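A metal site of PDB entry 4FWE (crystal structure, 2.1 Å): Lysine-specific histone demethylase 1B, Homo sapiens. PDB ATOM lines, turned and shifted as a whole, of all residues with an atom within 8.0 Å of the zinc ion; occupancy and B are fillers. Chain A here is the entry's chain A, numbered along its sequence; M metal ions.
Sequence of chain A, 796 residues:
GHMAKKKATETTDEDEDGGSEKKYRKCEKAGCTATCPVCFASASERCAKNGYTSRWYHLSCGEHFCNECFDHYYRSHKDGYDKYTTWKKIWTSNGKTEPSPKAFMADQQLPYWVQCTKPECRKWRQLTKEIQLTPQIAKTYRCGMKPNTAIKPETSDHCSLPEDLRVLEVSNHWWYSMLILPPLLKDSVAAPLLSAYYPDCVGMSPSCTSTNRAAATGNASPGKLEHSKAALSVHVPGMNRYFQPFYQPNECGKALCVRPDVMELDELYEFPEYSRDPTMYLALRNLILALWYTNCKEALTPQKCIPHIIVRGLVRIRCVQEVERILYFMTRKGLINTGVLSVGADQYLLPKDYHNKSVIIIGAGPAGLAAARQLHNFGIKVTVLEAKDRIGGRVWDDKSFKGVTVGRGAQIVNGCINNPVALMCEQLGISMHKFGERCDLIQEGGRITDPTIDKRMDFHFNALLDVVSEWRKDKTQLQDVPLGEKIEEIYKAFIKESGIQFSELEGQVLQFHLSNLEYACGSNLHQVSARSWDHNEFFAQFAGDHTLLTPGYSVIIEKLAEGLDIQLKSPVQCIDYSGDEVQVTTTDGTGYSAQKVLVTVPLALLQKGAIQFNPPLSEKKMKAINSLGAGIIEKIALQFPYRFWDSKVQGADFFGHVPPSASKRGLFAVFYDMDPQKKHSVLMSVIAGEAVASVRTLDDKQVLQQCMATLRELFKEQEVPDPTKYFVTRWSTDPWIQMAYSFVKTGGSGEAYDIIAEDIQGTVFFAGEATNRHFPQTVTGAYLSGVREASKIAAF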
ATOM      1  N   GLN A 115     -11.565 -20.883  14.822  1.00  0.00           N
ATOM      2  CA  GLN A 115     -11.638 -20.232  16.131  1.00  0.00           C
ATOM      3  C   GLN A 115     -13.086 -19.958  16.542  1.00  0.00           C
ATOM      4  O   GLN A 115     -13.886 -19.432  15.750  1.00  0.00           O
ATOM      5  CB  GLN A 115     -10.839 -18.938  16.130  1.00  0.00           C
ATOM      6  CG  GLN A 115     -10.674 -18.306  17.488  1.00  0.00           C
ATOM      7  CD  GLN A 115      -9.667 -17.175  17.487  1.00  0.00           C
ATOM      8  OE1 GLN A 115      -9.200 -16.741  18.539  1.00  0.00           O
ATOM      9  NE2 GLN A 115      -9.311 -16.697  16.305  1.00  0.00           N
ATOM     10  N   CYS A 116     -13.423 -20.299  17.781  1.00  0.00           N
ATOM     11  CA  CYS A 116     -14.767 -20.068  18.289  1.00  0.00           C
ATOM     12  C   CYS A 116     -15.034 -18.581  18.289  1.00  0.00           C
ATOM     13  O   CYS A 116     -14.208 -17.809  18.773  1.00  0.00           O
ATOM     14  CB  CYS A 116     -14.912 -20.615  19.709  1.00  0.00           C
ATOM     15  SG  CYS A 116     -16.562 -20.342  20.391  1.00  0.00           S
ATOM     16  N   THR A 117     -16.185 -18.191  17.759  1.00  0.00           N
ATOM     17  CA  THR A 117     -16.546 -16.778  17.625  1.00  0.00           C
ATOM     18  C   THR A 117     -17.302 -16.209  18.852  1.00  0.00           C
ATOM     19  O   THR A 117     -17.618 -15.029  18.896  1.00  0.00           O
ATOM     20  CB  THR A 117     -17.306 -16.478  16.302  1.00  0.00           C
ATOM     21  OG1 THR A 117     -18.495 -17.277  16.213  1.00  0.00           O
ATOM     22  CG2 THR A 117     -16.419 -16.807  15.101  1.00  0.00           C
ATOM     23  N   LYS A 118     -17.571 -17.057  19.848  1.00  0.00           N
ATOM     24  CA  LYS A 118     -18.071 -16.574  21.128  1.00  0.00           C
ATOM     25  C   LYS A 118     -16.953 -15.736  21.771  1.00  0.00           C
ATOM     26  O   LYS A 118     -15.838 -16.219  21.927  1.00  0.00           O
ATOM     27  CB  LYS A 118     -18.492 -17.739  22.025  1.00  0.00           C
ATOM     28  CG  LYS A 118     -18.913 -17.317  23.422  1.00  0.00           C
ATOM     29  CD  LYS A 118     -19.748 -18.392  24.094  1.00  0.00           C
ATOM     30  CE  LYS A 118     -20.133 -17.956  25.507  1.00  0.00           C
ATOM     31  NZ  LYS A 118     -21.353 -18.671  25.987  1.00  0.00           N
ATOM     32  N   PRO A 119     -17.265 -14.461  22.108  1.00  0.00           N
ATOM     33  CA  PRO A 119     -16.244 -13.520  22.595  1.00  0.00           C
ATOM     34  C   PRO A 119     -15.627 -13.947  23.911  1.00  0.00           C
ATOM     35  O   PRO A 119     -14.486 -13.603  24.186  1.00  0.00           O
ATOM     36  CB  PRO A 119     -17.031 -12.216  22.788  1.00  0.00           C
ATOM     37  CG  PRO A 119     -18.259 -12.378  21.956  1.00  0.00           C
ATOM     38  CD  PRO A 119     -18.590 -13.829  22.033  1.00  0.00           C
ATOM     39  N   GLU A 120     -16.371 -14.702  24.711  1.00  0.00           N
ATOM     40  CA  GLU A 120     -15.898 -15.138  26.013  1.00  0.00           C
ATOM     41  C   GLU A 120     -15.046 -16.398  25.867  1.00  0.00           C
ATOM     42  O   GLU A 120     -14.423 -16.831  26.831  1.00  0.00           O
ATOM     43  CB  GLU A 120     -17.071 -15.413  26.959  1.00  0.00           C
ATOM     44  N   CYS A 121     -15.041 -16.973  24.665  1.00  0.00           N
ATOM     45  CA  CYS A 121     -14.390 -18.266  24.433  1.00  0.00           C
ATOM     46  C   CYS A 121     -13.138 -18.135  23.560  1.00  0.00           C
ATOM     47  O   CYS A 121     -12.020 -18.235  24.064  1.00  0.00           O
ATOM     48  CB  CYS A 121     -15.374 -19.274  23.829  1.00  0.00           C
ATOM     49  SG  CYS A 121     -14.638 -20.866  23.405  1.00  0.00           S
ATOM     50  N   ARG A 122     -13.334 -17.896  22.267  1.00  0.00           N
ATOM     51  CA  ARG A 122     -12.241 -17.681  21.302  1.00  0.00           C
ATOM     52  C   ARG A 122     -11.276 -18.864  21.222  1.00  0.00           C
ATOM     53  O   ARG A 122     -10.119 -18.690  20.833  1.00  0.00           O
ATOM     54  CB  ARG A 122     -11.472 -16.376  21.583  1.00  0.00           C
ATOM     55  CG  ARG A 122     -12.342 -15.176  21.921  1.00  0.00           C
ATOM     56  CD  ARG A 122     -12.678 -14.297  20.721  1.00  0.00           C
ATOM     57  NE  ARG A 122     -13.115 -15.042  19.545  1.00  0.00           N
ATOM     58  CZ  ARG A 122     -12.494 -15.001  18.372  1.00  0.00           C
ATOM     59  NH1 ARG A 122     -11.418 -14.229  18.226  1.00  0.00           N
ATOM     60  NH2 ARG A 122     -12.950 -15.723  17.353  1.00  0.00           N
ATOM     61  N   LYS A 123     -11.731 -20.055  21.601  1.00  0.00           N
ATOM     62  CA  LYS A 123     -10.851 -21.211  21.497  1.00  0.00           C
ATOM     63  C   LYS A 123     -10.753 -21.672  20.063  1.00  0.00           C
ATOM     64  O   LYS A 123     -11.740 -21.658  19.324  1.00  0.00           O
ATOM     65  CB  LYS A 123     -11.324 -22.364  22.390  1.00  0.00           C
ATOM     66  CG  LYS A 123     -10.922 -22.192  23.848  1.00  0.00           C
ATOM     67  CD  LYS A 123     -11.568 -23.237  24.740  1.00  0.00           C
ATOM     68  CE  LYS A 123     -11.361 -22.883  26.198  1.00  0.00           C
ATOM     69  NZ  LYS A 123     -12.306 -23.632  27.063  1.00  0.00           N
ATOM     70  N   TRP A 124      -9.553 -22.071  19.673  1.00  0.00           N
ATOM     71  CA  TRP A 124      -9.297 -22.704  18.402  1.00  0.00           C
ATOM     72  C   TRP A 124      -9.608 -24.170  18.463  1.00  0.00           C
ATOM     73  O   TRP A 124      -9.146 -24.856  19.371  1.00  0.00           O
ATOM     74  CB  TRP A 124      -7.841 -22.539  18.041  1.00  0.00           C
ATOM     75  CG  TRP A 124      -7.529 -21.197  17.425  1.00  0.00           C
ATOM     76  CD1 TRP A 124      -7.085 -20.033  18.062  1.00  0.00           C
ATOM     77  CD2 TRP A 124      -7.661 -20.835  16.020  1.00  0.00           C
ATOM     78  NE1 TRP A 124      -6.920 -19.013  17.156  1.00  0.00           N
ATOM     79  CE2 TRP A 124      -7.242 -19.429  15.911  1.00  0.00           C
ATOM     80  CE3 TRP A 124      -8.052 -21.519  14.872  1.00  0.00           C
ATOM     81  CZ2 TRP A 124      -7.222 -18.770  14.695  1.00  0.00           C
ATOM     82  CZ3 TRP A 124      -8.028 -20.830  13.653  1.00  0.00           C
ATOM     83  CH2 TRP A 124      -7.626 -19.487  13.575  1.00  0.00           C
ATOM     84  N   ARG A 125     -10.374 -24.656  17.489  1.00  0.00           N
ATOM     85  CA  ARG A 125     -10.736 -26.059  17.375  1.00  0.00           C
ATOM     86  C   ARG A 125     -10.281 -26.666  16.067  1.00  0.00           C
ATOM     87  O   ARG A 125     -10.369 -26.021  14.997  1.00  0.00           O
ATOM     88  CB  ARG A 125     -12.251 -26.236  17.487  1.00  0.00           C
ATOM     89  CG  ARG A 125     -12.848 -25.762  18.797  1.00  0.00           C
ATOM     90  CD  ARG A 125     -12.171 -26.338  20.039  1.00  0.00           C
ATOM     91  NE  ARG A 125     -12.928 -25.959  21.239  1.00  0.00           N
ATOM     92  CZ  ARG A 125     -12.555 -26.216  22.503  1.00  0.00           C
ATOM     93  NH1 ARG A 125     -11.426 -26.870  22.764  1.00  0.00           N
ATOM     94  NH2 ARG A 125     -13.345 -25.839  23.496  1.00  0.00           N
ATOM     95  N   TYR A 141     -18.585 -19.939  13.501  1.00  0.00           N
ATOM     96  CA  TYR A 141     -18.149 -21.065  14.337  1.00  0.00           C
ATOM     97  C   TYR A 141     -18.293 -20.881  15.867  1.00  0.00           C
ATOM     98  O   TYR A 141     -17.843 -19.880  16.445  1.00  0.00           O
ATOM     99  CB  TYR A 141     -16.732 -21.536  13.994  1.00  0.00           C
ATOM    100  CG  TYR A 141     -16.411 -22.808  14.747  1.00  0.00           C
ATOM    101  CD1 TYR A 141     -16.968 -24.025  14.357  1.00  0.00           C
ATOM    102  CD2 TYR A 141     -15.596 -22.779  15.869  1.00  0.00           C
ATOM    103  CE1 TYR A 141     -16.696 -25.181  15.060  1.00  0.00           C
ATOM    104  CE2 TYR A 141     -15.310 -23.932  16.571  1.00  0.00           C
ATOM    105  CZ  TYR A 141     -15.859 -25.129  16.156  1.00  0.00           C
ATOM    106  OH  TYR A 141     -15.587 -26.285  16.859  1.00  0.00           O
ATOM    107  N   ARG A 142     -18.914 -21.874  16.491  1.00  0.00           N
ATOM    108  CA  ARG A 142     -18.939 -21.966  17.946  1.00  0.00           C
ATOM    109  C   ARG A 142     -18.571 -23.397  18.342  1.00  0.00           C
ATOM    110  O   ARG A 142     -18.950 -24.344  17.647  1.00  0.00           O
ATOM    111  CB  ARG A 142     -20.308 -21.523  18.521  1.00  0.00           C
ATOM    112  CG  ARG A 142     -20.391 -20.018  18.798  1.00  0.00           C
ATOM    113  CD  ARG A 142     -21.804 -19.528  19.076  1.00  0.00           C
ATOM    114  NE  ARG A 142     -22.612 -19.489  17.851  1.00  0.00           N
ATOM    115  CZ  ARG A 142     -23.925 -19.277  17.792  1.00  0.00           C
ATOM    116  NH1 ARG A 142     -24.642 -19.078  18.898  1.00  0.00           N
ATOM    117  NH2 ARG A 142     -24.548 -19.279  16.621  1.00  0.00           N
ATOM    118  N   CYS A 143     -17.817 -23.553  19.429  1.00  0.00           N
ATOM    119  CA  CYS A 143     -17.341 -24.888  19.867  1.00  0.00           C
ATOM    120  C   CYS A 143     -18.472 -25.892  19.858  1.00  0.00           C
ATOM    121  O   CYS A 143     -19.580 -25.589  20.319  1.00  0.00           O
ATOM    122  CB  CYS A 143     -16.714 -24.848  21.268  1.00  0.00           C
ATOM    123  SG  CYS A 143     -15.309 -23.714  21.469  1.00  0.00           S
ATOM    124  N   GLY A 144     -18.188 -27.056  19.302  1.00  0.00           N
ATOM    125  CA  GLY A 144     -19.165 -28.137  19.245  1.00  0.00           C
ATOM    126  C   GLY A 144     -20.111 -28.110  18.054  1.00  0.00           C
ATOM    127  O   GLY A 144     -20.928 -29.013  17.910  1.00  0.00           O
ATOM    128  N   SER A 156     -23.767 -23.380  25.775  1.00  0.00           N
ATOM    129  CA  SER A 156     -22.408 -23.133  25.293  1.00  0.00           C
ATOM    130  C   SER A 156     -21.355 -23.813  26.174  1.00  0.00           C
ATOM    131  O   SER A 156     -20.318 -23.223  26.495  1.00  0.00           O
ATOM    132  CB  SER A 156     -22.147 -21.627  25.172  1.00  0.00           C
ATOM    133  N   ASP A 157     -21.623 -25.064  26.551  1.00  0.00           N
ATOM    134  CA  ASP A 157     -20.740 -25.827  27.428  1.00  0.00           C
ATOM    135  C   ASP A 157     -19.572 -26.483  26.696  1.00  0.00           C
ATOM    136  O   ASP A 157     -18.520 -26.715  27.277  1.00  0.00           O
ATOM    137  CB  ASP A 157     -21.508 -26.852  28.272  1.00  0.00           C
ATOM    138  CG  ASP A 157     -22.287 -27.859  27.421  1.00  0.00           C
ATOM    139  OD1 ASP A 157     -23.387 -28.265  27.854  1.00  0.00           O
ATOM    140  OD2 ASP A 157     -21.794 -28.245  26.343  1.00  0.00           O
ATOM    141  N   HIS A 158     -19.775 -26.800  25.413  1.00  0.00           N
ATOM    142  CA  HIS A 158     -18.689 -27.247  24.531  1.00  0.00           C
ATOM    143  C   HIS A 158     -17.515 -26.302  24.534  1.00  0.00           C
ATOM    144  O   HIS A 158     -16.390 -26.709  24.273  1.00  0.00           O
ATOM    145  CB  HIS A 158     -19.197 -27.388  23.110  1.00  0.00           C
ATOM    146  CG  HIS A 158     -19.629 -28.786  22.738  1.00  0.00           C
ATOM    147  ND1 HIS A 158     -20.926 -29.150  22.681  1.00  0.00           N
ATOM    148  CD2 HIS A 158     -18.885 -29.895  22.347  1.00  0.00           C
ATOM    149  CE1 HIS A 158     -20.998 -30.442  22.301  1.00  0.00           C
ATOM    150  NE2 HIS A 158     -19.753 -30.899  22.090  1.00  0.00           N
ATOM    151  N   CYS A 159     -17.784 -25.022  24.811  1.00  0.00           N
ATOM    152  CA  CYS A 159     -16.727 -24.002  24.931  1.00  0.00           C
ATOM    153  C   CYS A 159     -15.756 -24.262  26.092  1.00  0.00           C
ATOM    154  O   CYS A 159     -14.619 -23.807  26.049  1.00  0.00           O
ATOM    155  CB  CYS A 159     -17.340 -22.617  25.099  1.00  0.00           C
ATOM    156  SG  CYS A 159     -18.112 -21.925  23.618  1.00  0.00           S
ATOM    157  N   SER A 160     -16.225 -24.972  27.118  1.00  0.00           N
ATOM    158  CA  SER A 160     -15.436 -25.159  28.330  1.00  0.00           C
ATOM    159  C   SER A 160     -14.408 -26.287  28.229  1.00  0.00           C
ATOM    160  O   SER A 160     -13.495 -26.376  29.043  1.00  0.00           O
ATOM    161  CB  SER A 160     -16.361 -25.367  29.540  1.00  0.00           C
ATOM    162  OG  SER A 160     -16.991 -26.636  29.482  1.00  0.00           O
ATOM    163  N   LEU A 161     -14.545 -27.167  27.241  1.00  0.00           N
ATOM    164  CA  LEU A 161     -13.528 -28.174  26.952  1.00  0.00           C
ATOM    165  C   LEU A 161     -12.185 -27.475  26.681  1.00  0.00           C
ATOM    166  O   LEU A 161     -12.154 -26.475  25.949  1.00  0.00           O
ATOM    167  CB  LEU A 161     -13.925 -29.029  25.754  1.00  0.00           C
ATOM    168  CG  LEU A 161     -15.308 -29.704  25.788  1.00  0.00           C
ATOM    169  CD1 LEU A 161     -15.310 -30.934  24.899  1.00  0.00           C
ATOM    170  CD2 LEU A 161     -15.734 -30.083  27.201  1.00  0.00           C
HETATM  171 ZN    ZN M   1     -16.172 -21.779  22.251  1.00  0.00          ZN
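O of Cys 116 sits at hydrogen-bond distance from NH2 of Arg 122 (2.8 Å).
The backbone NH (N) of Lys 123 lies close to the side-chain sulfur (SG) of Cys 121 (3.5 Å).
SG of Cys 143 lies close to NE of Arg 125 (3.3 Å).
SG of Cys 116 sits close to N of Lys 118 (3.5 Å).
The backbone carbonyl oxygen (O) of Lys 123 lies within hydrogen-bond range of the backbone NH (N) of Cys 116 (2.7 Å).
The backbone carbonyl oxygen (O) of Cys 159 lies within hydrogen-bond range of the side-chain amino group (NZ) of Lys 123, at 2.5 Å.
Of the 21 residues printed, 4 come within 4 Å of the zinc ion.
The zinc ion is bound by SG of Cys 121 (2.1 Å), SG of Cys 143 (2.3 Å), SG of Cys 159 (2.4 Å) and SG of Cys 116 (2.4 Å).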
